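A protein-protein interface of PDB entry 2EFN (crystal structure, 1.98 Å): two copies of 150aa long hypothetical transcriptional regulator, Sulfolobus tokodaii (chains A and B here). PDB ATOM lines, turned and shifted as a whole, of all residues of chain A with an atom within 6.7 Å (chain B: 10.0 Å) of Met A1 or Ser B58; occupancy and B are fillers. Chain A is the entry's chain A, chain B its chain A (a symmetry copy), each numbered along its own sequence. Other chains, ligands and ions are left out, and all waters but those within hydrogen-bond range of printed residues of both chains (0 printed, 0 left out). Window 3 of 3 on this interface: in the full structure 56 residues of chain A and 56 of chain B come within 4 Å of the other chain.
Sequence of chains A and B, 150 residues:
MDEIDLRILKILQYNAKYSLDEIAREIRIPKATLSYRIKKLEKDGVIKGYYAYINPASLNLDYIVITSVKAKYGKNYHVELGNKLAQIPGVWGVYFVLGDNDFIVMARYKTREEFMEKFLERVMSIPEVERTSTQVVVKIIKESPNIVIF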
ATOM      1  N   MET A   1      -9.491 -18.144   6.411  1.00  0.00           N
ATOM      2  CA  MET A   1      -9.635 -19.376   5.581  1.00  0.00           C
ATOM      3  C   MET A   1      -8.966 -19.198   4.219  1.00  0.00           C
ATOM      4  O   MET A   1      -8.610 -18.081   3.835  1.00  0.00           O
ATOM      5  CB  MET A   1     -11.118 -19.711   5.405  1.00  0.00           C
ATOM      6  CG  MET A   1     -11.941 -18.600   4.781  1.00  0.00           C
ATOM      7  SD  MET A   1     -13.706 -18.964   4.788  1.00  0.00           S
ATOM      8  CE  MET A   1     -14.207 -18.152   6.299  1.00  0.00           C
ATOM      9  N   ASP A   2      -8.796 -20.301   3.496  1.00  0.00           N
ATOM     10  CA  ASP A   2      -8.153 -20.263   2.190  1.00  0.00           C
ATOM     11  C   ASP A   2      -9.092 -20.578   1.027  1.00  0.00           C
ATOM     12  O   ASP A   2     -10.306 -20.707   1.199  1.00  0.00           O
ATOM     13  CB  ASP A   2      -6.968 -21.232   2.155  1.00  0.00           C
ATOM     14  CG  ASP A   2      -7.347 -22.637   2.583  1.00  0.00           C
ATOM     15  OD1 ASP A   2      -8.375 -23.155   2.095  1.00  0.00           O
ATOM     16  OD2 ASP A   2      -6.611 -23.227   3.403  1.00  0.00           O
ATOM     17  N   GLU A   3      -8.508 -20.694  -0.160  1.00  0.00           N
ATOM     18  CA  GLU A   3      -9.261 -20.978  -1.375  1.00  0.00           C
ATOM     19  C   GLU A   3      -9.999 -22.313  -1.289  1.00  0.00           C
ATOM     20  O   GLU A   3     -11.109 -22.452  -1.811  1.00  0.00           O
ATOM     21  CB  GLU A   3      -8.314 -20.994  -2.576  1.00  0.00           C
ATOM     22  CG  GLU A   3      -7.167 -21.988  -2.415  1.00  0.00           C
ATOM     23  CD  GLU A   3      -6.426 -22.260  -3.710  1.00  0.00           C
ATOM     24  OE1 GLU A   3      -5.786 -21.328  -4.250  1.00  0.00           O
ATOM     25  OE2 GLU A   3      -6.482 -23.416  -4.185  1.00  0.00           O
ATOM     26  N   ILE A   4      -9.380 -23.292  -0.639  1.00  0.00           N
ATOM     27  CA  ILE A   4      -9.994 -24.604  -0.499  1.00  0.00           C
ATOM     28  C   ILE A   4     -11.261 -24.504   0.345  1.00  0.00           C
ATOM     29  O   ILE A   4     -12.278 -25.118   0.017  1.00  0.00           O
ATOM     30  CB  ILE A   4      -9.007 -25.621   0.123  1.00  0.00           C
ATOM     31  CG1 ILE A   4      -7.869 -25.899  -0.865  1.00  0.00           C
ATOM     32  CG2 ILE A   4      -9.724 -26.918   0.471  1.00  0.00           C
ATOM     33  CD1 ILE A   4      -6.810 -26.851  -0.341  1.00  0.00           C
ATOM     34  N   ASP A   5     -11.212 -23.725   1.422  1.00  0.00           N
ATOM     35  CA  ASP A   5     -12.391 -23.554   2.267  1.00  0.00           C
ATOM     36  C   ASP A   5     -13.518 -22.947   1.437  1.00  0.00           C
ATOM     37  O   ASP A   5     -14.674 -23.355   1.542  1.00  0.00           O
ATOM     38  CB  ASP A   5     -12.088 -22.639   3.455  1.00  0.00           C
ATOM     39  CG  ASP A   5     -11.089 -23.246   4.413  1.00  0.00           C
ATOM     40  OD1 ASP A   5     -11.278 -24.418   4.809  1.00  0.00           O
ATOM     41  OD2 ASP A   5     -10.119 -22.550   4.776  1.00  0.00           O
ATOM     42  N   LEU A   6     -13.165 -21.976   0.602  1.00  0.00           N
ATOM     43  CA  LEU A   6     -14.138 -21.305  -0.252  1.00  0.00           C
ATOM     44  C   LEU A   6     -14.818 -22.263  -1.222  1.00  0.00           C
ATOM     45  O   LEU A   6     -16.026 -22.165  -1.458  1.00  0.00           O
ATOM     46  CB  LEU A   6     -13.459 -20.178  -1.027  1.00  0.00           C
ATOM     47  CG  LEU A   6     -12.958 -19.031  -0.147  1.00  0.00           C
ATOM     48  CD1 LEU A   6     -12.297 -17.971  -1.011  1.00  0.00           C
ATOM     49  CD2 LEU A   6     -14.127 -18.438   0.633  1.00  0.00           C
ATOM     50  N   LEU A   9     -17.241 -24.302   0.836  1.00  0.00           N
ATOM     51  CA  LEU A   9     -18.426 -23.521   1.166  1.00  0.00           C
ATOM     52  C   LEU A   9     -19.296 -23.321  -0.074  1.00  0.00           C
ATOM     53  O   LEU A   9     -20.526 -23.336   0.006  1.00  0.00           O
ATOM     54  CB  LEU A   9     -18.013 -22.161   1.740  1.00  0.00           C
ATOM     55  CG  LEU A   9     -17.313 -22.184   3.101  1.00  0.00           C
ATOM     56  CD1 LEU A   9     -16.778 -20.801   3.435  1.00  0.00           C
ATOM     57  CD2 LEU A   9     -18.295 -22.656   4.165  1.00  0.00           C
ATOM     58  N   ARG A  37     -11.457 -29.735   7.734  1.00  0.00           N
ATOM     59  CA  ARG A  37     -11.714 -28.366   7.308  1.00  0.00           C
ATOM     60  C   ARG A  37     -13.147 -27.933   7.590  1.00  0.00           C
ATOM     61  O   ARG A  37     -13.383 -26.804   8.014  1.00  0.00           O
ATOM     62  CB  ARG A  37     -11.403 -28.211   5.819  1.00  0.00           C
ATOM     63  CG  ARG A  37      -9.924 -28.027   5.518  1.00  0.00           C
ATOM     64  CD  ARG A  37      -9.637 -28.165   4.040  1.00  0.00           C
ATOM     65  NE  ARG A  37      -8.299 -27.691   3.705  1.00  0.00           N
ATOM     66  CZ  ARG A  37      -7.964 -26.408   3.609  1.00  0.00           C
ATOM     67  NH1 ARG A  37      -8.873 -25.463   3.814  1.00  0.00           N
ATOM     68  NH2 ARG A  37      -6.714 -26.068   3.316  1.00  0.00           N
ATOM     69  N   LEU A  41     -14.455 -24.974  10.096  1.00  0.00           N
ATOM     70  CA  LEU A  41     -15.294 -23.863   9.660  1.00  0.00           C
ATOM     71  C   LEU A  41     -16.482 -23.688  10.601  1.00  0.00           C
ATOM     72  O   LEU A  41     -16.896 -22.567  10.890  1.00  0.00           O
ATOM     73  CB  LEU A  41     -15.796 -24.100   8.231  1.00  0.00           C
ATOM     74  CG  LEU A  41     -14.727 -24.059   7.135  1.00  0.00           C
ATOM     75  CD1 LEU A  41     -15.320 -24.529   5.811  1.00  0.00           C
ATOM     76  CD2 LEU A  41     -14.174 -22.642   7.014  1.00  0.00           C
ATOM     77  N   ASP A  44     -15.155 -22.196  13.867  1.00  0.00           N
ATOM     78  CA  ASP A  44     -14.757 -20.798  13.741  1.00  0.00           C
ATOM     79  C   ASP A  44     -15.932 -19.873  13.457  1.00  0.00           C
ATOM     80  O   ASP A  44     -15.747 -18.682  13.206  1.00  0.00           O
ATOM     81  CB  ASP A  44     -13.697 -20.637  12.649  1.00  0.00           C
ATOM     82  CG  ASP A  44     -12.413 -21.375  12.975  1.00  0.00           C
ATOM     83  OD1 ASP A  44     -12.189 -21.670  14.167  1.00  0.00           O
ATOM     84  OD2 ASP A  44     -11.624 -21.651  12.045  1.00  0.00           O
ATOM     85  N   GLY A  45     -17.141 -20.421  13.490  1.00  0.00           N
ATOM     86  CA  GLY A  45     -18.321 -19.611  13.250  1.00  0.00           C
ATOM     87  C   GLY A  45     -18.611 -19.266  11.799  1.00  0.00           C
ATOM     88  O   GLY A  45     -19.487 -18.445  11.528  1.00  0.00           O
ATOM     89  N   VAL A  46     -17.886 -19.873  10.864  1.00  0.00           N
ATOM     90  CA  VAL A  46     -18.125 -19.608   9.447  1.00  0.00           C
ATOM     91  C   VAL A  46     -19.414 -20.320   9.045  1.00  0.00           C
ATOM     92  O   VAL A  46     -20.315 -19.716   8.461  1.00  0.00           O
ATOM     93  CB  VAL A  46     -16.963 -20.107   8.584  1.00  0.00           C
ATOM     94  CG1 VAL A  46     -17.242 -19.815   7.115  1.00  0.00           C
ATOM     95  CG2 VAL A  46     -15.674 -19.432   9.029  1.00  0.00           C
ATOM     96  N   ILE A  47     -19.487 -21.613   9.345  1.00  0.00           N
ATOM     97  CA  ILE A  47     -20.693 -22.380   9.073  1.00  0.00           C
ATOM     98  C   ILE A  47     -21.489 -22.321  10.373  1.00  0.00           C
ATOM     99  O   ILE A  47     -21.089 -22.911  11.373  1.00  0.00           O
ATOM    100  CB  ILE A  47     -20.385 -23.856   8.745  1.00  0.00           C
ATOM    101  CG1 ILE A  47     -19.594 -23.946   7.437  1.00  0.00           C
ATOM    102  CG2 ILE A  47     -21.687 -24.639   8.648  1.00  0.00           C
ATOM    103  CD1 ILE A  47     -19.200 -25.351   7.041  1.00  0.00           C
ATOM    104  N   LYS A  48     -22.605 -21.601  10.354  1.00  0.00           N
ATOM    105  CA  LYS A  48     -23.452 -21.435  11.532  1.00  0.00           C
ATOM    106  C   LYS A  48     -24.350 -22.637  11.808  1.00  0.00           C
ATOM    107  O   LYS A  48     -24.743 -22.880  12.951  1.00  0.00           O
ATOM    108  CB  LYS A  48     -24.318 -20.186  11.370  1.00  0.00           C
ATOM    109  CG  LYS A  48     -23.529 -18.896  11.176  1.00  0.00           C
ATOM    110  CD  LYS A  48     -22.866 -18.442  12.466  1.00  0.00           C
ATOM    111  CE  LYS A  48     -23.905 -18.017  13.494  1.00  0.00           C
ATOM    112  NZ  LYS A  48     -23.285 -17.582  14.774  1.00  0.00           N
ATOM    113  N   TYR B  53     -25.652 -22.866   6.535  1.00  0.00           N
ATOM    114  CA  TYR B  53     -25.867 -21.441   6.754  1.00  0.00           C
ATOM    115  C   TYR B  53     -24.506 -20.818   7.007  1.00  0.00           C
ATOM    116  O   TYR B  53     -23.859 -21.094   8.015  1.00  0.00           O
ATOM    117  CB  TYR B  53     -26.773 -21.170   7.954  1.00  0.00           C
ATOM    118  CG  TYR B  53     -27.087 -19.695   8.095  1.00  0.00           C
ATOM    119  CD1 TYR B  53     -27.868 -19.038   7.141  1.00  0.00           C
ATOM    120  CD2 TYR B  53     -26.563 -18.944   9.145  1.00  0.00           C
ATOM    121  CE1 TYR B  53     -28.116 -17.669   7.229  1.00  0.00           C
ATOM    122  CE2 TYR B  53     -26.804 -17.572   9.243  1.00  0.00           C
ATOM    123  CZ  TYR B  53     -27.580 -16.941   8.281  1.00  0.00           C
ATOM    124  OH  TYR B  53     -27.823 -15.587   8.368  1.00  0.00           O
ATOM    125  N   ILE B  54     -24.075 -19.980   6.076  1.00  0.00           N
ATOM    126  CA  ILE B  54     -22.778 -19.336   6.180  1.00  0.00           C
ATOM    127  C   ILE B  54     -22.884 -17.899   6.657  1.00  0.00           C
ATOM    128  O   ILE B  54     -23.710 -17.132   6.169  1.00  0.00           O
ATOM    129  CB  ILE B  54     -22.064 -19.353   4.823  1.00  0.00           C
ATOM    130  CG1 ILE B  54     -21.935 -20.796   4.333  1.00  0.00           C
ATOM    131  CG2 ILE B  54     -20.694 -18.691   4.939  1.00  0.00           C
ATOM    132  CD1 ILE B  54     -21.318 -20.914   2.965  1.00  0.00           C
ATOM    133  N   ASN B  55     -22.033 -17.546   7.613  1.00  0.00           N
ATOM    134  CA  ASN B  55     -22.006 -16.201   8.160  1.00  0.00           C
ATOM    135  C   ASN B  55     -21.424 -15.233   7.127  1.00  0.00           C
ATOM    136  O   ASN B  55     -20.239 -15.295   6.800  1.00  0.00           O
ATOM    137  CB  ASN B  55     -21.168 -16.180   9.437  1.00  0.00           C
ATOM    138  CG  ASN B  55     -20.959 -14.781   9.970  1.00  0.00           C
ATOM    139  OD1 ASN B  55     -21.885 -13.974   9.995  1.00  0.00           O
ATOM    140  ND2 ASN B  55     -19.742 -14.489  10.407  1.00  0.00           N
ATOM    141  N   PRO B  56     -22.260 -14.326   6.599  1.00  0.00           N
ATOM    142  CA  PRO B  56     -21.852 -13.335   5.597  1.00  0.00           C
ATOM    143  C   PRO B  56     -20.598 -12.553   5.977  1.00  0.00           C
ATOM    144  O   PRO B  56     -19.780 -12.220   5.119  1.00  0.00           O
ATOM    145  CB  PRO B  56     -23.082 -12.439   5.486  1.00  0.00           C
ATOM    146  CG  PRO B  56     -24.204 -13.405   5.716  1.00  0.00           C
ATOM    147  CD  PRO B  56     -23.695 -14.187   6.908  1.00  0.00           C
ATOM    148  N   ALA B  57     -20.448 -12.267   7.266  1.00  0.00           N
ATOM    149  CA  ALA B  57     -19.292 -11.521   7.745  1.00  0.00           C
ATOM    150  C   ALA B  57     -18.016 -12.310   7.504  1.00  0.00           C
ATOM    151  O   ALA B  57     -16.974 -11.739   7.182  1.00  0.00           O
ATOM    152  CB  ALA B  57     -19.441 -11.210   9.226  1.00  0.00           C
ATOM    153  N   SER B  58     -18.104 -13.629   7.656  1.00  0.00           N
ATOM    154  CA  SER B  58     -16.952 -14.497   7.454  1.00  0.00           C
ATOM    155  C   SER B  58     -16.419 -14.369   6.041  1.00  0.00           C
ATOM    156  O   SER B  58     -15.256 -14.679   5.776  1.00  0.00           O
ATOM    157  CB  SER B  58     -17.325 -15.956   7.728  1.00  0.00           C
ATOM    158  OG  SER B  58     -17.618 -16.152   9.098  1.00  0.00           O
ATOM    159  N   LEU B  59     -17.279 -13.919   5.132  1.00  0.00           N
ATOM    160  CA  LEU B  59     -16.902 -13.744   3.742  1.00  0.00           C
ATOM    161  C   LEU B  59     -16.723 -12.263   3.444  1.00  0.00           C
ATOM    162  O   LEU B  59     -16.647 -11.858   2.287  1.00  0.00           O
ATOM    163  CB  LEU B  59     -17.973 -14.345   2.827  1.00  0.00           C
ATOM    164  CG  LEU B  59     -18.144 -15.863   2.954  1.00  0.00           C
ATOM    165  CD1 LEU B  59     -19.434 -16.309   2.293  1.00  0.00           C
ATOM    166  CD2 LEU B  59     -16.945 -16.551   2.328  1.00  0.00           C
ATOM    167  N   ASN B  60     -16.670 -11.462   4.506  1.00  0.00           N
ATOM    168  CA  ASN B  60     -16.485 -10.018   4.398  1.00  0.00           C
ATOM    169  C   ASN B  60     -17.575  -9.312   3.592  1.00  0.00           C
ATOM    170  O   ASN B  60     -17.323  -8.284   2.964  1.00  0.00           O
ATOM    171  CB  ASN B  60     -15.111  -9.719   3.792  1.00  0.00           C
ATOM    172  CG  ASN B  60     -13.972 -10.171   4.690  1.00  0.00           C
ATOM    173  OD1 ASN B  60     -12.992 -10.748   4.224  1.00  0.00           O
ATOM    174  ND2 ASN B  60     -14.096  -9.906   5.986  1.00  0.00           N
ATOM    175  N   LEU B  61     -18.782  -9.868   3.601  1.00  0.00           N
ATOM    176  CA  LEU B  61     -19.900  -9.258   2.884  1.00  0.00           C
ATOM    177  C   LEU B  61     -20.402  -8.141   3.796  1.00  0.00           C
ATOM    178  O   LEU B  61     -21.341  -8.317   4.573  1.00  0.00           O
ATOM    179  CB  LEU B  61     -20.990 -10.304   2.626  1.00  0.00           C
ATOM    180  CG  LEU B  61     -20.519 -11.419   1.685  1.00  0.00           C
ATOM    181  CD1 LEU B  61     -21.548 -12.549   1.630  1.00  0.00           C
ATOM    182  CD2 LEU B  61     -20.273 -10.832   0.299  1.00  0.00           C
ATOM    183  N   ASP B  62     -19.741  -6.994   3.693  1.00  0.00           N
ATOM    184  CA  ASP B  62     -20.027  -5.838   4.528  1.00  0.00           C
ATOM    185  C   ASP B  62     -20.958  -4.801   3.907  1.00  0.00           C
ATOM    186  O   ASP B  62     -21.525  -3.970   4.619  1.00  0.00           O
ATOM    187  CB  ASP B  62     -18.705  -5.164   4.902  1.00  0.00           C
ATOM    188  CG  ASP B  62     -18.845  -4.209   6.066  1.00  0.00           C
ATOM    189  OD1 ASP B  62     -18.355  -3.069   5.957  1.00  0.00           O
ATOM    190  OD2 ASP B  62     -19.438  -4.603   7.092  1.00  0.00           O
ATOM    191  N   ILE B  64     -24.278  -4.405   2.310  1.00  0.00           N
ATOM    192  CA  ILE B  64     -25.589  -5.006   2.096  1.00  0.00           C
ATOM    193  C   ILE B  64     -26.560  -3.941   1.609  1.00  0.00           C
ATOM    194  O   ILE B  64     -26.675  -2.868   2.209  1.00  0.00           O
ATOM    195  CB  ILE B  64     -26.103  -5.625   3.413  1.00  0.00           C
ATOM    196  CG1 ILE B  64     -25.005  -6.500   4.031  1.00  0.00           C
ATOM    197  CG2 ILE B  64     -27.351  -6.459   3.158  1.00  0.00           C
ATOM    198  CD1 ILE B  64     -24.445  -7.560   3.090  1.00  0.00           C
ATOM    199  N   ARG B 108     -25.748  -8.532  -1.714  1.00  0.00           N
ATOM    200  CA  ARG B 108     -24.659  -8.446  -0.748  1.00  0.00           C
ATOM    201  C   ARG B 108     -23.327  -8.333  -1.483  1.00  0.00           C
ATOM    202  O   ARG B 108     -23.093  -9.048  -2.457  1.00  0.00           O
ATOM    203  CB  ARG B 108     -24.605  -9.703   0.125  1.00  0.00           C
ATOM    204  CG  ARG B 108     -25.887 -10.098   0.841  1.00  0.00           C
ATOM    205  CD  ARG B 108     -25.568 -11.237   1.800  1.00  0.00           C
ATOM    206  NE  ARG B 108     -26.737 -11.852   2.423  1.00  0.00           N
ATOM    207  CZ  ARG B 108     -27.275 -13.004   2.030  1.00  0.00           C
ATOM    208  NH1 ARG B 108     -26.754 -13.669   1.007  1.00  0.00           N
ATOM    209  NH2 ARG B 108     -28.321 -13.505   2.677  1.00  0.00           N
ATOM    210  N   LYS B 110     -18.842  -7.229  -0.770  1.00  0.00           N
ATOM    211  CA  LYS B 110     -17.793  -7.040   0.233  1.00  0.00           C
ATOM    212  C   LYS B 110     -17.545  -5.558   0.505  1.00  0.00           C
ATOM    213  O   LYS B 110     -17.310  -5.164   1.647  1.00  0.00           O
ATOM    214  CB  LYS B 110     -16.469  -7.647  -0.241  1.00  0.00           C
ATOM    215  CG  LYS B 110     -16.533  -9.112  -0.630  1.00  0.00           C
ATOM    216  CD  LYS B 110     -15.282  -9.509  -1.404  1.00  0.00           C
ATOM    217  CE  LYS B 110     -14.518 -10.628  -0.698  1.00  0.00           C
ATOM    218  NZ  LYS B 110     -15.280 -11.908  -0.604  1.00  0.00           N
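Met A1 touches Ser B58. Leu B59 touches Leu A6 (CD2 to CD2, 3.8 Å). Leu A9 touches Ile B54. CB of Asn B55 touches O of Gly A45, at 3.5 Å. Gly A45 touches Ser B58 (O to OG, 3.8 Å). Val A46 touches Tyr B53. O of Val A46 touches CA of Ile B54 (3.4 Å). CA of Val A46 touches OG of Ser B58, 3.5 Å away. Ile A47 touches Tyr B53 (C to O, 3.6 Å). CG of Lys A48 touches CB of Asn B55, at 3.997 Å.
O of Leu A41 is in hydrogen-bond range of N of Val A46 (2.9 Å). O of Leu A41 is in hydrogen-bond range of N of Ile A47 (3.2 Å). The side-chain amide nitrogen of Asn B55 lies within hydrogen-bond range of the side-chain hydroxyl of Ser B58 (3.0 Å). The backbone carbonyl oxygen (O) of Leu B59 lies within hydrogen-bond range of the side-chain amino group (NZ) of Lys B110, 3.2 Å away.
Hydrophobic or aromatic side chains of chain A within 4 Å of the printed part of chain B: Met A1, Leu A6, Leu A9 and Val A46. Of the 13 printed residues of chain B, 5 touch a printed residue of chain A. Printed residues of chain B that touch a printed residue of chain A: Tyr B53, Ile B54, Asn B55, Ser B58 and Leu B59. Hydrophobic or aromatic side chains of chain B within 4 Å of the printed part of chain A: Tyr B53, Ile B54 and Leu B59.
The backbone carbonyl oxygen of Val A46 lies within hydrogen-bond range of the backbone NH of Asn B55 (2.9 Å). N of Lys A48 sits at hydrogen-bond distance from O of Tyr B53, 2.7 Å away.
Met A1 touches just one residue of chain B: Ser B58 (3.7 Å). Ser B58 touches just these residues of chain A: Met A1, Gly A45 and Val A46. No residue of chain B comes within 4 Å of Asp A2. Val A46 touches just these residues of chain B: Tyr B53, Ile B54, Asn B55 and Ser B58. Of the printed residues of chain A, Leu B59 touches Leu A6. Of the printed residues of chain B, Lys A48 touches Tyr B53 and Asn B55. Printed residues of chain B within 4 Å of Ile A47: Tyr B53. Printed residues of chain A within 4 Å of Ile B54: Leu A9 (3.7 Å) and Val A46 (3.4 Å). Asn B60 touches none of the printed residues of chain A. Lys B110 touches none of the printed residues of chain A. The nearest residue of chain A that does not touch Ser B58 is Asp A44 (5.2 Å).
No position is printed for both chains.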
